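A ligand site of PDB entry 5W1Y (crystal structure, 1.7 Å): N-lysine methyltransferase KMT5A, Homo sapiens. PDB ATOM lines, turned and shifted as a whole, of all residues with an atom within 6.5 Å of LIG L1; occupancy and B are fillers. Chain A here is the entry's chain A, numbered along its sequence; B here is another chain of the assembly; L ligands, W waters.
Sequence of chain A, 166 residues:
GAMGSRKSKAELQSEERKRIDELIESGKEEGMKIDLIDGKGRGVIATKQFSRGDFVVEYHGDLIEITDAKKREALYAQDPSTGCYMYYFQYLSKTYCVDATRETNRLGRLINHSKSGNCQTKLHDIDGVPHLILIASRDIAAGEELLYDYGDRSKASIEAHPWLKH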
ATOM      1  N   GLU A  73      14.368 -23.374  -8.644  1.00  0.00           N
ATOM      2  CA  GLU A  73      15.232 -24.470  -8.944  1.00  0.00           C
ATOM      3  C   GLU A  73      15.780 -24.415 -10.365  1.00  0.00           C
ATOM      4  O   GLU A  73      16.927 -24.778 -10.589  1.00  0.00           O
ATOM      5  CB  GLU A  73      14.553 -25.836  -8.693  1.00  0.00           C
ATOM      6  CG  GLU A  73      14.412 -26.065  -7.194  1.00  0.00           C
ATOM      7  CD  GLU A  73      13.666 -27.324  -6.833  1.00  0.00           C
ATOM      8  OE1 GLU A  73      13.211 -28.035  -7.765  1.00  0.00           O
ATOM      9  OE2 GLU A  73      13.520 -27.561  -5.595  1.00  0.00           O
ATOM     10  N   TYR A  76      18.595 -21.807 -10.144  1.00  0.00           N
ATOM     11  CA  TYR A  76      19.749 -22.304  -9.417  1.00  0.00           C
ATOM     12  C   TYR A  76      20.582 -23.327 -10.219  1.00  0.00           C
ATOM     13  O   TYR A  76      21.828 -23.360 -10.100  1.00  0.00           O
ATOM     14  CB  TYR A  76      19.329 -22.865  -8.084  1.00  0.00           C
ATOM     15  CG  TYR A  76      18.723 -21.840  -7.129  1.00  0.00           C
ATOM     16  CD1 TYR A  76      19.149 -20.500  -7.133  1.00  0.00           C
ATOM     17  CD2 TYR A  76      17.755 -22.188  -6.241  1.00  0.00           C
ATOM     18  CE1 TYR A  76      18.615 -19.595  -6.231  1.00  0.00           C
ATOM     19  CE2 TYR A  76      17.223 -21.299  -5.358  1.00  0.00           C
ATOM     20  CZ  TYR A  76      17.663 -19.988  -5.356  1.00  0.00           C
ATOM     21  OH  TYR A  76      17.148 -19.076  -4.469  1.00  0.00           O
ATOM     22  N   ALA A  77      19.900 -24.097 -11.051  1.00  0.00           N
ATOM     23  CA  ALA A  77      20.521 -25.099 -11.903  1.00  0.00           C
ATOM     24  C   ALA A  77      21.469 -24.462 -12.939  1.00  0.00           C
ATOM     25  O   ALA A  77      22.423 -25.086 -13.378  1.00  0.00           O
ATOM     26  CB  ALA A  77      19.440 -25.919 -12.593  1.00  0.00           C
ATOM     27  N   GLN A  78      21.227 -23.194 -13.287  1.00  0.00           N
ATOM     28  CA  GLN A  78      22.174 -22.430 -14.112  1.00  0.00           C
ATOM     29  C   GLN A  78      23.442 -21.914 -13.406  1.00  0.00           C
ATOM     30  O   GLN A  78      24.412 -21.573 -14.079  1.00  0.00           O
ATOM     31  CB  GLN A  78      21.437 -21.240 -14.735  1.00  0.00           C
ATOM     32  CG  GLN A  78      20.280 -21.623 -15.629  1.00  0.00           C
ATOM     33  CD  GLN A  78      19.420 -20.426 -16.014  1.00  0.00           C
ATOM     34  OE1 GLN A  78      19.907 -19.288 -16.104  1.00  0.00           O
ATOM     35  NE2 GLN A  78      18.128 -20.666 -16.234  1.00  0.00           N
ATOM     36  N   ASP A  79      23.457 -21.806 -12.086  1.00  0.00           N
ATOM     37  CA  ASP A  79      24.584 -21.298 -11.360  1.00  0.00           C
ATOM     38  C   ASP A  79      25.245 -22.475 -10.619  1.00  0.00           C
ATOM     39  O   ASP A  79      24.788 -22.860  -9.561  1.00  0.00           O
ATOM     40  CB  ASP A  79      24.119 -20.206 -10.367  1.00  0.00           C
ATOM     41  CG  ASP A  79      25.210 -19.747  -9.391  1.00  0.00           C
ATOM     42  OD1 ASP A  79      26.355 -20.241  -9.429  1.00  0.00           O
ATOM     43  OD2 ASP A  79      24.914 -18.867  -8.557  1.00  0.00           O
ATOM     44  N   PRO A  80      26.342 -23.008 -11.150  1.00  0.00           N
ATOM     45  CA  PRO A  80      26.956 -24.171 -10.531  1.00  0.00           C
ATOM     46  C   PRO A  80      27.462 -24.091  -9.107  1.00  0.00           C
ATOM     47  O   PRO A  80      27.756 -25.127  -8.556  1.00  0.00           O
ATOM     48  CB  PRO A  80      28.149 -24.492 -11.469  1.00  0.00           C
ATOM     49  CG  PRO A  80      27.689 -24.011 -12.778  1.00  0.00           C
ATOM     50  CD  PRO A  80      26.916 -22.749 -12.490  1.00  0.00           C
ATOM     51  N   SER A  81      27.559 -22.910  -8.517  1.00  0.00           N
ATOM     52  CA  SER A  81      28.060 -22.778  -7.162  1.00  0.00           C
ATOM     53  C   SER A  81      26.941 -22.968  -6.124  1.00  0.00           C
ATOM     54  O   SER A  81      27.250 -23.076  -4.915  1.00  0.00           O
ATOM     55  CB  SER A  81      28.681 -21.403  -6.970  1.00  0.00           C
ATOM     56  OG  SER A  81      27.707 -20.414  -7.309  1.00  0.00           O
ATOM     57  N   THR A  82      25.687 -22.988  -6.581  1.00  0.00           N
ATOM     58  CA  THR A  82      24.541 -23.205  -5.665  1.00  0.00           C
ATOM     59  C   THR A  82      24.547 -24.644  -5.104  1.00  0.00           C
ATOM     60  O   THR A  82      24.819 -25.587  -5.836  1.00  0.00           O
ATOM     61  CB  THR A  82      23.170 -22.893  -6.323  1.00  0.00           C
ATOM     62  OG1 THR A  82      22.918 -23.707  -7.472  1.00  0.00           O
ATOM     63  CG2 THR A  82      23.114 -21.395  -6.725  1.00  0.00           C
ATOM     64  N   GLY A  83      24.302 -24.751  -3.809  1.00  0.00           N
ATOM     65  CA  GLY A  83      24.057 -26.024  -3.131  1.00  0.00           C
ATOM     66  C   GLY A  83      22.548 -26.288  -3.105  1.00  0.00           C
ATOM     67  O   GLY A  83      21.749 -25.602  -3.759  1.00  0.00           O
ATOM     68  N   CYS A  84      22.185 -27.328  -2.376  1.00  0.00           N
ATOM     69  CA  CYS A  84      20.809 -27.782  -2.266  1.00  0.00           C
ATOM     70  C   CYS A  84      20.274 -27.352  -0.903  1.00  0.00           C
ATOM     71  O   CYS A  84      20.495 -28.052   0.096  1.00  0.00           O
ATOM     72  CB  CYS A  84      20.714 -29.296  -2.410  1.00  0.00           C
ATOM     73  SG  CYS A  84      21.564 -29.832  -3.939  1.00  0.00           S
ATOM     74  N   TYR A  85      19.568 -26.245  -0.885  1.00  0.00           N
ATOM     75  CA  TYR A  85      19.116 -25.649   0.362  1.00  0.00           C
ATOM     76  C   TYR A  85      17.629 -25.348   0.386  1.00  0.00           C
ATOM     77  O   TYR A  85      17.167 -24.550   1.207  1.00  0.00           O
ATOM     78  CB  TYR A  85      19.945 -24.410   0.671  1.00  0.00           C
ATOM     79  CG  TYR A  85      21.435 -24.677   0.826  1.00  0.00           C
ATOM     80  CD1 TYR A  85      21.921 -25.421   1.894  1.00  0.00           C
ATOM     81  CD2 TYR A  85      22.340 -24.240  -0.106  1.00  0.00           C
ATOM     82  CE1 TYR A  85      23.256 -25.677   2.064  1.00  0.00           C
ATOM     83  CE2 TYR A  85      23.700 -24.462   0.071  1.00  0.00           C
ATOM     84  CZ  TYR A  85      24.161 -25.210   1.161  1.00  0.00           C
ATOM     85  OH  TYR A  85      25.510 -25.448   1.322  1.00  0.00           O
ATOM     86  N   THR A 101      19.051 -21.019  -0.204  1.00  0.00           N
ATOM     87  CA  THR A 101      20.122 -21.163  -1.201  1.00  0.00           C
ATOM     88  C   THR A 101      21.010 -19.872  -1.202  1.00  0.00           C
ATOM     89  O   THR A 101      22.217 -19.961  -1.428  1.00  0.00           O
ATOM     90  CB  THR A 101      19.503 -21.371  -2.590  1.00  0.00           C
ATOM     91  OG1 THR A 101      18.598 -22.488  -2.565  1.00  0.00           O
ATOM     92  CG2 THR A 101      20.582 -21.635  -3.634  1.00  0.00           C
ATOM     93  N   SER A 157      10.487 -33.029  -0.508  1.00  0.00           N
ATOM     94  CA  SER A 157      11.077 -32.727  -1.812  1.00  0.00           C
ATOM     95  C   SER A 157      10.571 -33.688  -2.903  1.00  0.00           C
ATOM     96  O   SER A 157      10.247 -33.274  -4.002  1.00  0.00           O
ATOM     97  CB  SER A 157      12.585 -32.772  -1.785  1.00  0.00           C
ATOM     98  OG  SER A 157      13.097 -32.270  -3.014  1.00  0.00           O
ATOM     99  N   HIS A 161       8.475 -33.035  -6.412  1.00  0.00           N
ATOM    100  CA  HIS A 161       9.162 -33.350  -7.656  1.00  0.00           C
ATOM    101  C   HIS A 161       8.723 -34.712  -8.188  1.00  0.00           C
ATOM    102  O   HIS A 161       9.390 -35.723  -7.963  1.00  0.00           O
ATOM    103  CB  HIS A 161      10.657 -33.373  -7.421  1.00  0.00           C
ATOM    104  CG  HIS A 161      11.211 -32.021  -7.132  1.00  0.00           C
ATOM    105  ND1 HIS A 161      11.521 -31.600  -5.840  1.00  0.00           N
ATOM    106  CD2 HIS A 161      11.506 -30.987  -7.943  1.00  0.00           C
ATOM    107  CE1 HIS A 161      11.976 -30.358  -5.896  1.00  0.00           C
ATOM    108  NE2 HIS A 161      11.977 -29.967  -7.165  1.00  0.00           N
ATOM    109  N   LEU A 164      11.087 -37.210  -9.660  1.00  0.00           N
ATOM    110  CA  LEU A 164      12.078 -37.894  -8.815  1.00  0.00           C
ATOM    111  C   LEU A 164      11.502 -39.104  -8.105  1.00  0.00           C
ATOM    112  O   LEU A 164      12.199 -39.703  -7.297  1.00  0.00           O
ATOM    113  CB  LEU A 164      12.725 -36.955  -7.770  1.00  0.00           C
ATOM    114  CG  LEU A 164      13.640 -35.917  -8.387  1.00  0.00           C
ATOM    115  CD1 LEU A 164      14.094 -34.918  -7.303  1.00  0.00           C
ATOM    116  CD2 LEU A 164      14.790 -36.546  -9.164  1.00  0.00           C
ATOM    117  N   THR B  82      23.491 -38.136  -0.021  1.00  0.00           N
ATOM    118  CA  THR B  82      24.071 -38.017  -1.341  1.00  0.00           C
ATOM    119  C   THR B  82      24.225 -36.572  -1.795  1.00  0.00           C
ATOM    120  O   THR B  82      23.358 -35.739  -1.533  1.00  0.00           O
ATOM    121  CB  THR B  82      23.262 -38.777  -2.398  1.00  0.00           C
ATOM    122  OG1 THR B  82      21.955 -38.203  -2.494  1.00  0.00           O
ATOM    123  CG2 THR B  82      23.261 -40.276  -2.097  1.00  0.00           C
ATOM    124  N   CYS B  84      25.408 -34.123  -5.475  1.00  0.00           N
ATOM    125  CA  CYS B  84      24.978 -34.056  -6.841  1.00  0.00           C
ATOM    126  C   CYS B  84      26.220 -34.359  -7.690  1.00  0.00           C
ATOM    127  O   CYS B  84      27.116 -33.483  -7.849  1.00  0.00           O
ATOM    128  CB  CYS B  84      24.398 -32.656  -7.171  1.00  0.00           C
ATOM    129  SG  CYS B  84      23.165 -32.131  -5.948  1.00  0.00           S
ATOM    130  N   SER B 154      26.373 -28.064 -16.295  1.00  0.00           N
ATOM    131  CA  SER B 154      25.123 -27.427 -15.923  1.00  0.00           C
ATOM    132  C   SER B 154      24.134 -27.468 -17.077  1.00  0.00           C
ATOM    133  O   SER B 154      22.995 -27.918 -16.908  1.00  0.00           O
ATOM    134  CB  SER B 154      25.383 -25.980 -15.537  1.00  0.00           C
ATOM    135  OG  SER B 154      24.156 -25.362 -15.293  1.00  0.00           O
ATOM    136  N   TRP B 163      12.031 -30.558 -17.053  1.00  0.00           N
ATOM    137  CA  TRP B 163      11.258 -29.916 -16.000  1.00  0.00           C
ATOM    138  C   TRP B 163      11.993 -28.775 -15.290  1.00  0.00           C
ATOM    139  O   TRP B 163      11.349 -27.926 -14.695  1.00  0.00           O
ATOM    140  CB  TRP B 163      10.739 -30.964 -14.976  1.00  0.00           C
ATOM    141  CG  TRP B 163      11.739 -31.975 -14.476  1.00  0.00           C
ATOM    142  CD1 TRP B 163      12.087 -33.170 -15.047  1.00  0.00           C
ATOM    143  CD2 TRP B 163      12.449 -31.898 -13.248  1.00  0.00           C
ATOM    144  NE1 TRP B 163      13.014 -33.804 -14.272  1.00  0.00           N
ATOM    145  CE2 TRP B 163      13.236 -33.051 -13.149  1.00  0.00           C
ATOM    146  CE3 TRP B 163      12.488 -30.965 -12.203  1.00  0.00           C
ATOM    147  CZ2 TRP B 163      14.039 -33.302 -12.073  1.00  0.00           C
ATOM    148  CZ3 TRP B 163      13.324 -31.210 -11.144  1.00  0.00           C
ATOM    149  CH2 TRP B 163      14.061 -32.373 -11.076  1.00  0.00           C
ATOM    150  N   LEU B 164      13.308 -28.742 -15.404  1.00  0.00           N
ATOM    151  CA  LEU B 164      14.115 -27.573 -15.014  1.00  0.00           C
ATOM    152  C   LEU B 164      14.256 -26.517 -16.146  1.00  0.00           C
ATOM    153  O   LEU B 164      15.108 -25.623 -16.043  1.00  0.00           O
ATOM    154  CB  LEU B 164      15.523 -28.033 -14.598  1.00  0.00           C
ATOM    155  CG  LEU B 164      15.688 -28.937 -13.378  1.00  0.00           C
ATOM    156  CD1 LEU B 164      17.142 -29.344 -13.232  1.00  0.00           C
ATOM    157  CD2 LEU B 164      15.259 -28.240 -12.108  1.00  0.00           C
HETATM  158  C1  LIG L   1      23.407 -28.058  -7.695  1.00  0.00           C
HETATM  159  C2  LIG L   1      22.773 -28.382  -6.390  1.00  0.00           C
HETATM  160  C3  LIG L   1      21.042 -26.676  -6.916  1.00  0.00           C
HETATM  161  C4  LIG L   1      21.737 -26.466  -8.222  1.00  0.00           C
HETATM  162  C5  LIG L   1      20.270 -29.792  -5.111  1.00  0.00           C
HETATM  163  C6  LIG L   1      16.934 -31.552  -5.659  1.00  0.00           C
HETATM  164  C7  LIG L   1      19.227 -29.048  -7.276  1.00  0.00           C
HETATM  165  O1  LIG L   1      19.308 -28.444  -8.305  1.00  0.00           O
HETATM  166  C8  LIG L   1      20.325 -28.947  -6.203  1.00  0.00           C
HETATM  167  N1  LIG L   1      21.356 -28.012  -6.388  1.00  0.00           N
HETATM  168  N2  LIG L   1      23.173 -26.660  -8.064  1.00  0.00           N
HETATM  169  C9  LIG L   1      23.880 -26.333  -9.296  1.00  0.00           C
HETATM  170  C10 LIG L   1      18.086 -29.919  -7.011  1.00  0.00           C
HETATM  171  C11 LIG L   1      17.023 -29.931  -7.900  1.00  0.00           C
HETATM  172  C12 LIG L   1      15.937 -30.754  -7.685  1.00  0.00           C
HETATM  173  C13 LIG L   1      15.901 -31.572  -6.576  1.00  0.00           C
HETATM  174  C14 LIG L   1      18.036 -30.727  -5.864  1.00  0.00           C
HETATM  175  C15 LIG L   1      19.173 -30.720  -4.898  1.00  0.00           C
HETATM  176  O2  LIG L   1      19.195 -31.509  -3.933  1.00  0.00           O
HETATM  177  C1  LG2 L   2      20.660 -34.029  -2.702  1.00  0.00           C
HETATM  178  C2  LG2 L   2      21.635 -33.664  -3.801  1.00  0.00           C
HETATM  179  C3  LG2 L   2      21.118 -35.763  -4.916  1.00  0.00           C
HETATM  180  C4  LG2 L   2      20.135 -36.070  -3.826  1.00  0.00           C
HETATM  181  C5  LG2 L   2      21.708 -32.633  -6.761  1.00  0.00           C
HETATM  182  C6  LG2 L   2      19.937 -31.942 -10.073  1.00  0.00           C
HETATM  183  C7  LG2 L   2      19.618 -33.990  -6.896  1.00  0.00           C
HETATM  184  O1  LG2 L   2      18.796 -34.749  -6.335  1.00  0.00           O
HETATM  185  C8  LG2 L   2      20.922 -33.642  -6.228  1.00  0.00           C
HETATM  186  N1  LG2 L   2      21.236 -34.308  -5.063  1.00  0.00           N
HETATM  187  N2  LG2 L   2      20.555 -35.486  -2.558  1.00  0.00           N
HETATM  188  C9  LG2 L   2      19.615 -35.833  -1.502  1.00  0.00           C
HETATM  189  C10 LG2 L   2      19.352 -33.406  -8.227  1.00  0.00           C
HETATM  190  C11 LG2 L   2      18.223 -33.826  -8.942  1.00  0.00           C
HETATM  191  C12 LG2 L   2      17.952 -33.299 -10.186  1.00  0.00           C
HETATM  192  C13 LG2 L   2      18.820 -32.385 -10.761  1.00  0.00           C
HETATM  193  C14 LG2 L   2      20.211 -32.435  -8.787  1.00  0.00           C
HETATM  194  C15 LG2 L   2      21.394 -31.947  -8.031  1.00  0.00           C
HETATM  195  O2  LG2 L   2      22.112 -30.975  -8.438  1.00  0.00           O
HETATM  196  O   HOH W   1      26.886 -27.719  -9.504  1.00  0.00           O
HETATM  197  O   HOH W   2      16.747 -34.798  -4.862  1.00  0.00           O
HETATM  198  O   HOH W   3      18.048 -26.001  -8.791  1.00  0.00           O
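Glu 73 touches LIG L1 (OE1 to C12, 3.9 Å). Tyr 76 touches LIG L1. O of Asp 79 touches C9 of LIG L1, 3.6 Å away. Pro 80 touches LIG L1. Gly 83 touches LIG L1. Leu 164 of chain A touches LIG L1. Cys 84 of chain B touches LIG L1. Hydrophobic or aromatic side chains within 4 Å of LIG L1: Leu 164 of chain A. Within 4 Å of LIG L1: Glu 73, Tyr 76, Asp 79, Pro 80, Thr 82 of chain A, Gly 83, Cys 84 of chain A, Leu 164 of chain A and Cys 84 of chain B.
O of Asp 79 sits at hydrogen-bond distance from OG1 of Thr 82 of chain A (2.9 Å). OG1 of Thr 82 of chain A sits at hydrogen-bond distance from O of Tyr 76 (2.9 Å). The side-chain carboxylate (OD1) of Asp 79 sits at hydrogen-bond distance from the side-chain hydroxyl (OG) of Ser 81, 2.5 Å away. The side-chain carboxylate (OE2) of Glu 73 lies close to a ring nitrogen (NE2) of His 161, at 3.3 Å.
Water W3 lies within hydrogen-bond range of O of Glu 73, O1 of LIG L1 and N of Ala 77.
C5 of LIG L1 is bonded to SG of Cys 84 of chain A. O of Thr 82 of chain A lies close to N2 of LIG L1 (3.0 Å). OG1 of Thr 82 of chain A lies close to N2 of LIG L1, 3.0 Å away. SG of Cys 84 of chain B is bonded to C5 of LG2 L2, at 1.7 Å. O of Thr 82 of chain B sits close to N2 of LG2 L2 (3.0 Å). A nitrogen (N2) of LG2 L2 sits close to the side-chain hydroxyl (OG1) of Thr 82 of chain B, 3.1 Å away.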
